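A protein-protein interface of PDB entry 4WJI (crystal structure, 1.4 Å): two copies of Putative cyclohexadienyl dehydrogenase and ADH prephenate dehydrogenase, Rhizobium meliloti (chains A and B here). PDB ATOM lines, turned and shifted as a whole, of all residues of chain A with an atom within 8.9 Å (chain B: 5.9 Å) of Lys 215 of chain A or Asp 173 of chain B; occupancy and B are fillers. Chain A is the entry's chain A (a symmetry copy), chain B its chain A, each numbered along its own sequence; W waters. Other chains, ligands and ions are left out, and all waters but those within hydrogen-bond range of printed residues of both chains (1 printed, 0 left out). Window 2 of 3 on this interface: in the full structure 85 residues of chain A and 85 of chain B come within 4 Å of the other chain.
Printed residues of chain B within 4 Å of Lys 215 of chain A: Trp 144 and Asp 173.
Of the printed residues of chain B, Ser 217 of chain A touches Gln 291.
Of the printed residues of chain B, Ser 219 of chain A touches Ile 124.
Printed residues of chain A within 4 Å of Trp 144 of chain B: Lys 215 (3.1 Å) and Tyr 216 (3.8 Å).
No residue of chain A comes within 4 Å of Val 172 of chain B.
Glu 174 of chain B touches none of the printed residues of chain A.
Of the printed residues of chain A, Gln 291 of chain B touches Ile 214, Ser 217 and Arg 222.
The nearest residue of chain A that does not touch Asp 173 of chain B is Glu 212 of chain A (6.6 Å).
The nearest printed residue of chain B that does not touch Ser 219 of chain A is Gln 291 of chain B (7.0 Å).
Hydrophobic or aromatic side chains of chain A within 4 Å of the printed part of chain B: Tyr 216.
Of the 13 printed residues of chain B, 6 touch a printed residue of chain A.
Hydrophobic or aromatic side chains of chain B that line the printed part of chain A: Ile 124, Trp 144, Ile 146 and Met 175.
Among the printed residues, 11 pairs touch across the chains.
Among the printed residues, Asp or Glu carboxylates within 4 Å of a Lys or Arg side-chain nitrogen of the other chain: Lys 215 of chain A with Asp 173 of chain B (2.7 Å).
Water W1 lies within hydrogen-bond range of O of Lys 215 of chain A (2.7 Å), OE1 of Gln 291 of chain B (2.7 Å), N of Ala 218 of chain A (2.9 Å) and N of Ser 217 of chain A (3.4 Å).
NZ of Lys 215 of chain A is in salt-bridge range of OD2 of Asp 173 of chain B.
The side-chain carboxylate (OD2) of Asp 173 of chain B is in hydrogen-bond range of the side-chain hydroxyl (OH) of Tyr 216 of chain A, at 2.5 Å.
The backbone carbonyl oxygen (O) of Gln 291 of chain B sits at hydrogen-bond distance from the guanidinium group (NH1) of Arg 222 of chain A (3.0 Å).
The backbone NH of Ile 124 of chain B lies within hydrogen-bond range of the backbone carbonyl oxygen of Trp 144 of chain B (2.8 Å).
O of Cys 145 of chain B sits at hydrogen-bond distance from N of Asp 173 of chain B.
The backbone NH (N) of Leu 147 of chain B sits at hydrogen-bond distance from the backbone carbonyl oxygen (O) of Asp 173 of chain B, 2.9 Å away.
The backbone NH of Met 175 of chain B lies within hydrogen-bond range of the backbone carbonyl oxygen of Leu 147 of chain B.
The side-chain hydroxyl of Ser 217 of chain A sits at hydrogen-bond distance from the backbone carbonyl oxygen of Ile 214 of chain A, at 2.8 Å.
N of Arg 222 of chain A sits at hydrogen-bond distance from O of Ser 217 of chain A, 2.9 Å away.
Gln 291 of chain B touches Ile 214 of chain A.
Lys 215 of chain A touches Trp 144 of chain B.
CG2 of Ile 124 of chain B touches O of Tyr 216 of chain A, 3.5 Å away.
CD1 of Tyr 216 of chain A touches CB of Trp 144 of chain B, 3.8 Å away.
Ile 146 of chain B touches Tyr 216 of chain A (CD1 to CZ, 3.8 Å).
Tyr 216 of chain A touches Met 175 of chain B.
CB of Gln 291 of chain B touches OG of Ser 217 of chain A, at 3.7 Å.
CG2 of Ile 124 of chain B touches CB of Ser 219 of chain A (3.7 Å).
No position is printed for both chains.
Of the 11 pairs that touch across the chains among the printed residues, none has its exchanged pair printed and touching as well.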
ATOM      1  N   THR A 209      32.688  18.212  20.938  1.00  0.00           N
ATOM      2  CA  THR A 209      31.727  19.302  21.014  1.00  0.00           C
ATOM      3  C   THR A 209      30.961  19.290  22.319  1.00  0.00           C
ATOM      4  O   THR A 209      30.865  18.237  23.008  1.00  0.00           O
ATOM      5  CB  THR A 209      30.679  19.272  19.881  1.00  0.00           C
ATOM      6  OG1 THR A 209      29.814  18.131  20.025  1.00  0.00           O
ATOM      7  CG2 THR A 209      31.339  19.257  18.513  1.00  0.00           C
ATOM      8  N   GLU A 210      30.400  20.466  22.650  1.00  0.00           N
ATOM      9  CA  GLU A 210      29.482  20.613  23.805  1.00  0.00           C
ATOM     10  C   GLU A 210      28.318  19.607  23.712  1.00  0.00           C
ATOM     11  O   GLU A 210      27.953  18.950  24.681  1.00  0.00           O
ATOM     12  CB  GLU A 210      28.933  22.062  23.904  1.00  0.00           C
ATOM     13  N   SER A 211      27.758  19.470  22.519  1.00  0.00           N
ATOM     14  CA  SER A 211      26.683  18.519  22.287  1.00  0.00           C
ATOM     15  C   SER A 211      27.084  17.077  22.677  1.00  0.00           C
ATOM     16  O   SER A 211      26.306  16.364  23.330  1.00  0.00           O
ATOM     17  CB  SER A 211      26.247  18.594  20.822  1.00  0.00           C
ATOM     18  OG  SER A 211      25.154  17.737  20.594  1.00  0.00           O
ATOM     19  N   GLU A 212      28.280  16.644  22.281  1.00  0.00           N
ATOM     20  CA  GLU A 212      28.771  15.316  22.674  1.00  0.00           C
ATOM     21  C   GLU A 212      28.909  15.157  24.197  1.00  0.00           C
ATOM     22  O   GLU A 212      28.517  14.158  24.778  1.00  0.00           O
ATOM     23  CB  GLU A 212      30.106  15.022  21.970  1.00  0.00           C
ATOM     24  CG  GLU A 212      29.910  14.744  20.480  1.00  0.00           C
ATOM     25  CD  GLU A 212      31.190  14.658  19.654  1.00  0.00           C
ATOM     26  OE1 GLU A 212      32.172  15.409  19.901  1.00  0.00           O
ATOM     27  OE2 GLU A 212      31.201  13.840  18.715  1.00  0.00           O
ATOM     28  N   VAL A 213      29.476  16.156  24.848  1.00  0.00           N
ATOM     29  CA  VAL A 213      29.649  16.085  26.294  1.00  0.00           C
ATOM     30  C   VAL A 213      28.287  15.904  27.006  1.00  0.00           C
ATOM     31  O   VAL A 213      28.113  15.086  27.927  1.00  0.00           O
ATOM     32  CB  VAL A 213      30.412  17.313  26.804  1.00  0.00           C
ATOM     33  CG1 VAL A 213      30.449  17.306  28.316  1.00  0.00           C
ATOM     34  CG2 VAL A 213      31.832  17.323  26.273  1.00  0.00           C
ATOM     35  N   ILE A 214      27.290  16.638  26.547  1.00  0.00           N
ATOM     36  CA  ILE A 214      25.979  16.594  27.143  1.00  0.00           C
ATOM     37  C   ILE A 214      25.323  15.251  26.872  1.00  0.00           C
ATOM     38  O   ILE A 214      24.811  14.608  27.790  1.00  0.00           O
ATOM     39  CB  ILE A 214      25.073  17.744  26.574  1.00  0.00           C
ATOM     40  CG1 ILE A 214      25.648  19.113  26.938  1.00  0.00           C
ATOM     41  CG2 ILE A 214      23.650  17.597  27.043  1.00  0.00           C
ATOM     42  CD1 ILE A 214      25.177  20.197  26.006  1.00  0.00           C
ATOM     43  N   LYS A 215      25.292  14.842  25.588  1.00  0.00           N
ATOM     44  CA  LYS A 215      24.655  13.606  25.204  1.00  0.00           C
ATOM     45  C   LYS A 215      25.199  12.376  25.958  1.00  0.00           C
ATOM     46  O   LYS A 215      24.425  11.498  26.319  1.00  0.00           O
ATOM     47  CB  LYS A 215      24.802  13.339  23.694  1.00  0.00           C
ATOM     48  CG  LYS A 215      23.969  14.288  22.859  1.00  0.00           C
ATOM     49  CD  LYS A 215      24.362  14.308  21.397  1.00  0.00           C
ATOM     50  CE  LYS A 215      24.329  12.946  20.784  1.00  0.00           C
ATOM     51  NZ  LYS A 215      24.282  13.101  19.270  1.00  0.00           N
ATOM     52  N   TYR A 216      26.525  12.290  26.148  1.00  0.00           N
ATOM     53  CA  TYR A 216      27.153  11.089  26.660  1.00  0.00           C
ATOM     54  C   TYR A 216      27.552  11.218  28.116  1.00  0.00           C
ATOM     55  O   TYR A 216      28.320  10.379  28.660  1.00  0.00           O
ATOM     56  CB  TYR A 216      28.354  10.714  25.788  1.00  0.00           C
ATOM     57  CG  TYR A 216      28.022  10.616  24.278  1.00  0.00           C
ATOM     58  CD1 TYR A 216      26.891   9.967  23.795  1.00  0.00           C
ATOM     59  CD2 TYR A 216      28.843  11.242  23.346  1.00  0.00           C
ATOM     60  CE1 TYR A 216      26.622   9.923  22.431  1.00  0.00           C
ATOM     61  CE2 TYR A 216      28.575  11.183  22.001  1.00  0.00           C
ATOM     62  CZ  TYR A 216      27.460  10.559  21.557  1.00  0.00           C
ATOM     63  OH  TYR A 216      27.223  10.523  20.193  1.00  0.00           O
ATOM     64  N   SER A 217      26.980  12.226  28.786  1.00  0.00           N
ATOM     65  CA  SER A 217      27.341  12.507  30.177  1.00  0.00           C
ATOM     66  C   SER A 217      27.010  11.419  31.197  1.00  0.00           C
ATOM     67  O   SER A 217      27.611  11.419  32.295  1.00  0.00           O
ATOM     68  CB  SER A 217      26.730  13.853  30.607  1.00  0.00           C
ATOM     69  OG  SER A 217      25.313  13.828  30.480  1.00  0.00           O
ATOM     70  N   ALA A 218      26.108  10.492  30.859  1.00  0.00           N
ATOM     71  CA  ALA A 218      25.761   9.391  31.785  1.00  0.00           C
ATOM     72  C   ALA A 218      26.835   8.331  31.931  1.00  0.00           C
ATOM     73  O   ALA A 218      26.638   7.368  32.668  1.00  0.00           O
ATOM     74  CB  ALA A 218      24.413   8.756  31.426  1.00  0.00           C
ATOM     75  N   SER A 219      27.994   8.529  31.284  1.00  0.00           N
ATOM     76  CA  SER A 219      29.146   7.641  31.445  1.00  0.00           C
ATOM     77  C   SER A 219      30.099   8.115  32.537  1.00  0.00           C
ATOM     78  O   SER A 219      31.179   7.566  32.717  1.00  0.00           O
ATOM     79  CB  SER A 219      29.900   7.365  30.131  1.00  0.00           C
ATOM     80  OG  SER A 219      30.306   8.568  29.497  1.00  0.00           O
ATOM     81  N   PHE A 221      30.484  11.832  33.669  1.00  0.00           N
ATOM     82  CA  PHE A 221      30.679  13.255  33.747  1.00  0.00           C
ATOM     83  C   PHE A 221      29.533  13.923  34.485  1.00  0.00           C
ATOM     84  O   PHE A 221      29.772  14.882  35.239  1.00  0.00           O
ATOM     85  CB  PHE A 221      30.744  13.802  32.329  1.00  0.00           C
ATOM     86  CG  PHE A 221      31.172  15.223  32.204  1.00  0.00           C
ATOM     87  CD1 PHE A 221      32.488  15.596  32.341  1.00  0.00           C
ATOM     88  CD2 PHE A 221      30.245  16.177  31.805  1.00  0.00           C
ATOM     89  CE1 PHE A 221      32.857  16.936  32.195  1.00  0.00           C
ATOM     90  CE2 PHE A 221      30.610  17.488  31.629  1.00  0.00           C
ATOM     91  CZ  PHE A 221      31.903  17.859  31.825  1.00  0.00           C
ATOM     92  N   ARG A 222      28.312  13.447  34.296  1.00  0.00           N
ATOM     93  CA  ARG A 222      27.166  14.087  34.901  1.00  0.00           C
ATOM     94  C   ARG A 222      27.290  14.261  36.438  1.00  0.00           C
ATOM     95  O   ARG A 222      26.832  15.301  36.975  1.00  0.00           O
ATOM     96  CB  ARG A 222      25.844  13.438  34.502  1.00  0.00           C
ATOM     97  CG  ARG A 222      25.726  12.040  35.041  1.00  0.00           C
ATOM     98  CD  ARG A 222      24.393  11.409  34.606  1.00  0.00           C
ATOM     99  NE  ARG A 222      24.296  10.017  35.033  1.00  0.00           N
ATOM    100  CZ  ARG A 222      23.179   9.298  34.965  1.00  0.00           C
ATOM    101  NH1 ARG A 222      22.087   9.830  34.448  1.00  0.00           N
ATOM    102  NH2 ARG A 222      23.173   8.059  35.434  1.00  0.00           N
ATOM    103  N   ILE B 124      26.032   3.756  26.568  1.00  0.00           N
ATOM    104  CA  ILE B 124      26.448   4.842  27.478  1.00  0.00           C
ATOM    105  C   ILE B 124      25.525   4.792  28.675  1.00  0.00           C
ATOM    106  O   ILE B 124      24.696   5.664  28.884  1.00  0.00           O
ATOM    107  CB  ILE B 124      26.494   6.179  26.754  1.00  0.00           C
ATOM    108  CG1 ILE B 124      27.238   6.070  25.424  1.00  0.00           C
ATOM    109  CG2 ILE B 124      27.094   7.228  27.649  1.00  0.00           C
ATOM    110  CD1 ILE B 124      28.674   5.552  25.489  1.00  0.00           C
ATOM    111  N   TRP B 144      22.062   6.859  25.388  1.00  0.00           N
ATOM    112  CA  TRP B 144      22.701   6.758  24.108  1.00  0.00           C
ATOM    113  C   TRP B 144      23.521   5.474  24.008  1.00  0.00           C
ATOM    114  O   TRP B 144      23.991   4.935  25.033  1.00  0.00           O
ATOM    115  CB  TRP B 144      23.654   7.976  23.856  1.00  0.00           C
ATOM    116  CG  TRP B 144      22.896   9.193  23.520  1.00  0.00           C
ATOM    117  CD1 TRP B 144      22.421  10.134  24.407  1.00  0.00           C
ATOM    118  CD2 TRP B 144      22.495   9.601  22.250  1.00  0.00           C
ATOM    119  NE1 TRP B 144      21.716  11.098  23.737  1.00  0.00           N
ATOM    120  CE2 TRP B 144      21.732  10.776  22.406  1.00  0.00           C
ATOM    121  CE3 TRP B 144      22.650   9.057  20.971  1.00  0.00           C
ATOM    122  CZ2 TRP B 144      21.158  11.433  21.336  1.00  0.00           C
ATOM    123  CZ3 TRP B 144      22.067   9.719  19.915  1.00  0.00           C
ATOM    124  CH2 TRP B 144      21.335  10.893  20.107  1.00  0.00           C
ATOM    125  N   CYS B 145      23.655   4.986  22.768  1.00  0.00           N
ATOM    126  CA  CYS B 145      24.581   3.897  22.429  1.00  0.00           C
ATOM    127  C   CYS B 145      25.346   4.330  21.182  1.00  0.00           C
ATOM    128  O   CYS B 145      24.761   4.911  20.255  1.00  0.00           O
ATOM    129  CB  CYS B 145      23.834   2.601  22.190  1.00  0.00           C
ATOM    130  SG  CYS B 145      24.972   1.272  21.761  1.00  0.00           S
ATOM    131  N   ILE B 146      26.658   4.113  21.202  1.00  0.00           N
ATOM    132  CA  ILE B 146      27.519   4.502  20.092  1.00  0.00           C
ATOM    133  C   ILE B 146      27.998   3.248  19.375  1.00  0.00           C
ATOM    134  O   ILE B 146      28.575   2.344  19.984  1.00  0.00           O
ATOM    135  CB  ILE B 146      28.740   5.342  20.572  1.00  0.00           C
ATOM    136  CG1 ILE B 146      28.303   6.626  21.303  1.00  0.00           C
ATOM    137  CG2 ILE B 146      29.667   5.659  19.417  1.00  0.00           C
ATOM    138  CD1 ILE B 146      29.413   7.326  22.048  1.00  0.00           C
ATOM    139  N   LEU B 147      27.756   3.205  18.080  1.00  0.00           N
ATOM    140  CA  LEU B 147      28.339   2.176  17.205  1.00  0.00           C
ATOM    141  C   LEU B 147      29.522   2.714  16.447  1.00  0.00           C
ATOM    142  O   LEU B 147      29.520   3.879  16.037  1.00  0.00           O
ATOM    143  CB  LEU B 147      27.292   1.657  16.227  1.00  0.00           C
ATOM    144  CG  LEU B 147      25.974   1.127  16.784  1.00  0.00           C
ATOM    145  CD1 LEU B 147      25.030   0.636  15.675  1.00  0.00           C
ATOM    146  CD2 LEU B 147      26.238   0.053  17.824  1.00  0.00           C
ATOM    147  N   THR B 148      30.537   1.866  16.243  1.00  0.00           N
ATOM    148  CA  THR B 148      31.756   2.343  15.551  1.00  0.00           C
ATOM    149  C   THR B 148      32.147   1.331  14.419  1.00  0.00           C
ATOM    150  O   THR B 148      33.200   0.696  14.471  1.00  0.00           O
ATOM    151  CB  THR B 148      32.937   2.622  16.528  1.00  0.00           C
ATOM    152  OG1 THR B 148      33.402   1.393  17.100  1.00  0.00           O
ATOM    153  CG2 THR B 148      32.539   3.522  17.631  1.00  0.00           C
ATOM    154  N   ARG B 162      21.473  -1.245  15.079  1.00  0.00           N
ATOM    155  CA  ARG B 162      20.790   0.010  15.445  1.00  0.00           C
ATOM    156  C   ARG B 162      19.361  -0.286  15.919  1.00  0.00           C
ATOM    157  O   ARG B 162      18.927   0.223  16.969  1.00  0.00           O
ATOM    158  CB  ARG B 162      20.779   1.004  14.278  1.00  0.00           C
ATOM    159  CG  ARG B 162      19.947   2.232  14.518  1.00  0.00           C
ATOM    160  CD  ARG B 162      19.984   3.184  13.334  1.00  0.00           C
ATOM    161  NE  ARG B 162      21.291   3.780  13.138  1.00  0.00           N
ATOM    162  CZ  ARG B 162      21.679   4.958  13.641  1.00  0.00           C
ATOM    163  NH1 ARG B 162      20.837   5.698  14.362  1.00  0.00           N
ATOM    164  NH2 ARG B 162      22.909   5.413  13.421  1.00  0.00           N
ATOM    165  N   MET B 171      19.014   5.722  22.102  1.00  0.00           N
ATOM    166  CA  MET B 171      19.230   6.510  20.922  1.00  0.00           C
ATOM    167  C   MET B 171      20.598   6.093  20.434  1.00  0.00           C
ATOM    168  O   MET B 171      21.463   5.885  21.246  1.00  0.00           O
ATOM    169  CB  MET B 171      19.210   8.017  21.244  1.00  0.00           C
ATOM    170  CG  MET B 171      17.826   8.691  21.319  1.00  0.00           C
ATOM    171  SD  MET B 171      17.787  10.086  22.715  1.00  0.00           S
ATOM    172  CE  MET B 171      17.645   8.433  23.816  1.00  0.00           C
ATOM    173  N   VAL B 172      20.797   5.968  19.134  1.00  0.00           N
ATOM    174  CA  VAL B 172      22.018   5.459  18.552  1.00  0.00           C
ATOM    175  C   VAL B 172      22.744   6.483  17.664  1.00  0.00           C
ATOM    176  O   VAL B 172      22.135   7.107  16.837  1.00  0.00           O
ATOM    177  CB  VAL B 172      21.693   4.216  17.729  1.00  0.00           C
ATOM    178  CG1 VAL B 172      22.951   3.673  17.096  1.00  0.00           C
ATOM    179  CG2 VAL B 172      21.074   3.155  18.616  1.00  0.00           C
ATOM    180  N   ASP B 173      24.043   6.615  17.865  1.00  0.00           N
ATOM    181  CA  ASP B 173      24.916   7.431  17.035  1.00  0.00           C
ATOM    182  C   ASP B 173      26.032   6.553  16.503  1.00  0.00           C
ATOM    183  O   ASP B 173      26.434   5.632  17.143  1.00  0.00           O
ATOM    184  CB  ASP B 173      25.613   8.512  17.856  1.00  0.00           C
ATOM    185  CG  ASP B 173      24.865   9.794  17.917  1.00  0.00           C
ATOM    186  OD1 ASP B 173      24.076  10.061  17.037  1.00  0.00           O
ATOM    187  OD2 ASP B 173      25.071  10.564  18.894  1.00  0.00           O
ATOM    188  N   GLU B 174      26.538   6.872  15.336  1.00  0.00           N
ATOM    189  CA  GLU B 174      27.696   6.196  14.760  1.00  0.00           C
ATOM    190  C   GLU B 174      28.864   7.150  14.694  1.00  0.00           C
ATOM    191  O   GLU B 174      28.678   8.308  14.358  1.00  0.00           O
ATOM    192  CB  GLU B 174      27.376   5.716  13.345  1.00  0.00           C
ATOM    193  CG  GLU B 174      26.164   4.816  13.284  1.00  0.00           C
ATOM    194  CD  GLU B 174      25.783   4.384  11.872  1.00  0.00           C
ATOM    195  OE1 GLU B 174      26.671   4.208  11.007  1.00  0.00           O
ATOM    196  OE2 GLU B 174      24.578   4.184  11.669  1.00  0.00           O
ATOM    197  N   MET B 175      30.051   6.662  14.994  1.00  0.00           N
ATOM    198  CA  MET B 175      31.257   7.459  14.845  1.00  0.00           C
ATOM    199  C   MET B 175      32.471   6.617  14.608  1.00  0.00           C
ATOM    200  O   MET B 175      32.454   5.427  14.764  1.00  0.00           O
ATOM    201  CB  MET B 175      31.500   8.458  15.984  1.00  0.00           C
ATOM    202  CG  MET B 175      31.794   7.738  17.281  1.00  0.00           C
ATOM    203  SD  MET B 175      31.765   8.985  18.841  1.00  0.00           S
ATOM    204  CE  MET B 175      29.887   9.450  18.840  1.00  0.00           C
ATOM    205  N   GLN B 291      19.383  14.001  30.774  1.00  0.00           N
ATOM    206  CA  GLN B 291      20.478  13.065  31.046  1.00  0.00           C
ATOM    207  C   GLN B 291      20.940  13.067  32.479  1.00  0.00           C
ATOM    208  O   GLN B 291      21.823  12.306  32.806  1.00  0.00           O
ATOM    209  CB  GLN B 291      21.643  13.256  30.092  1.00  0.00           C
ATOM    210  CG  GLN B 291      21.382  12.840  28.632  1.00  0.00           C
ATOM    211  CD  GLN B 291      21.000  11.387  28.506  1.00  0.00           C
ATOM    212  OE1 GLN B 291      21.620  10.537  29.103  1.00  0.00           O
ATOM    213  NE2 GLN B 291      19.931  11.107  27.789  1.00  0.00           N
HETATM  214  O   HOH W   1      24.266  10.239  28.677  1.00  0.00           O
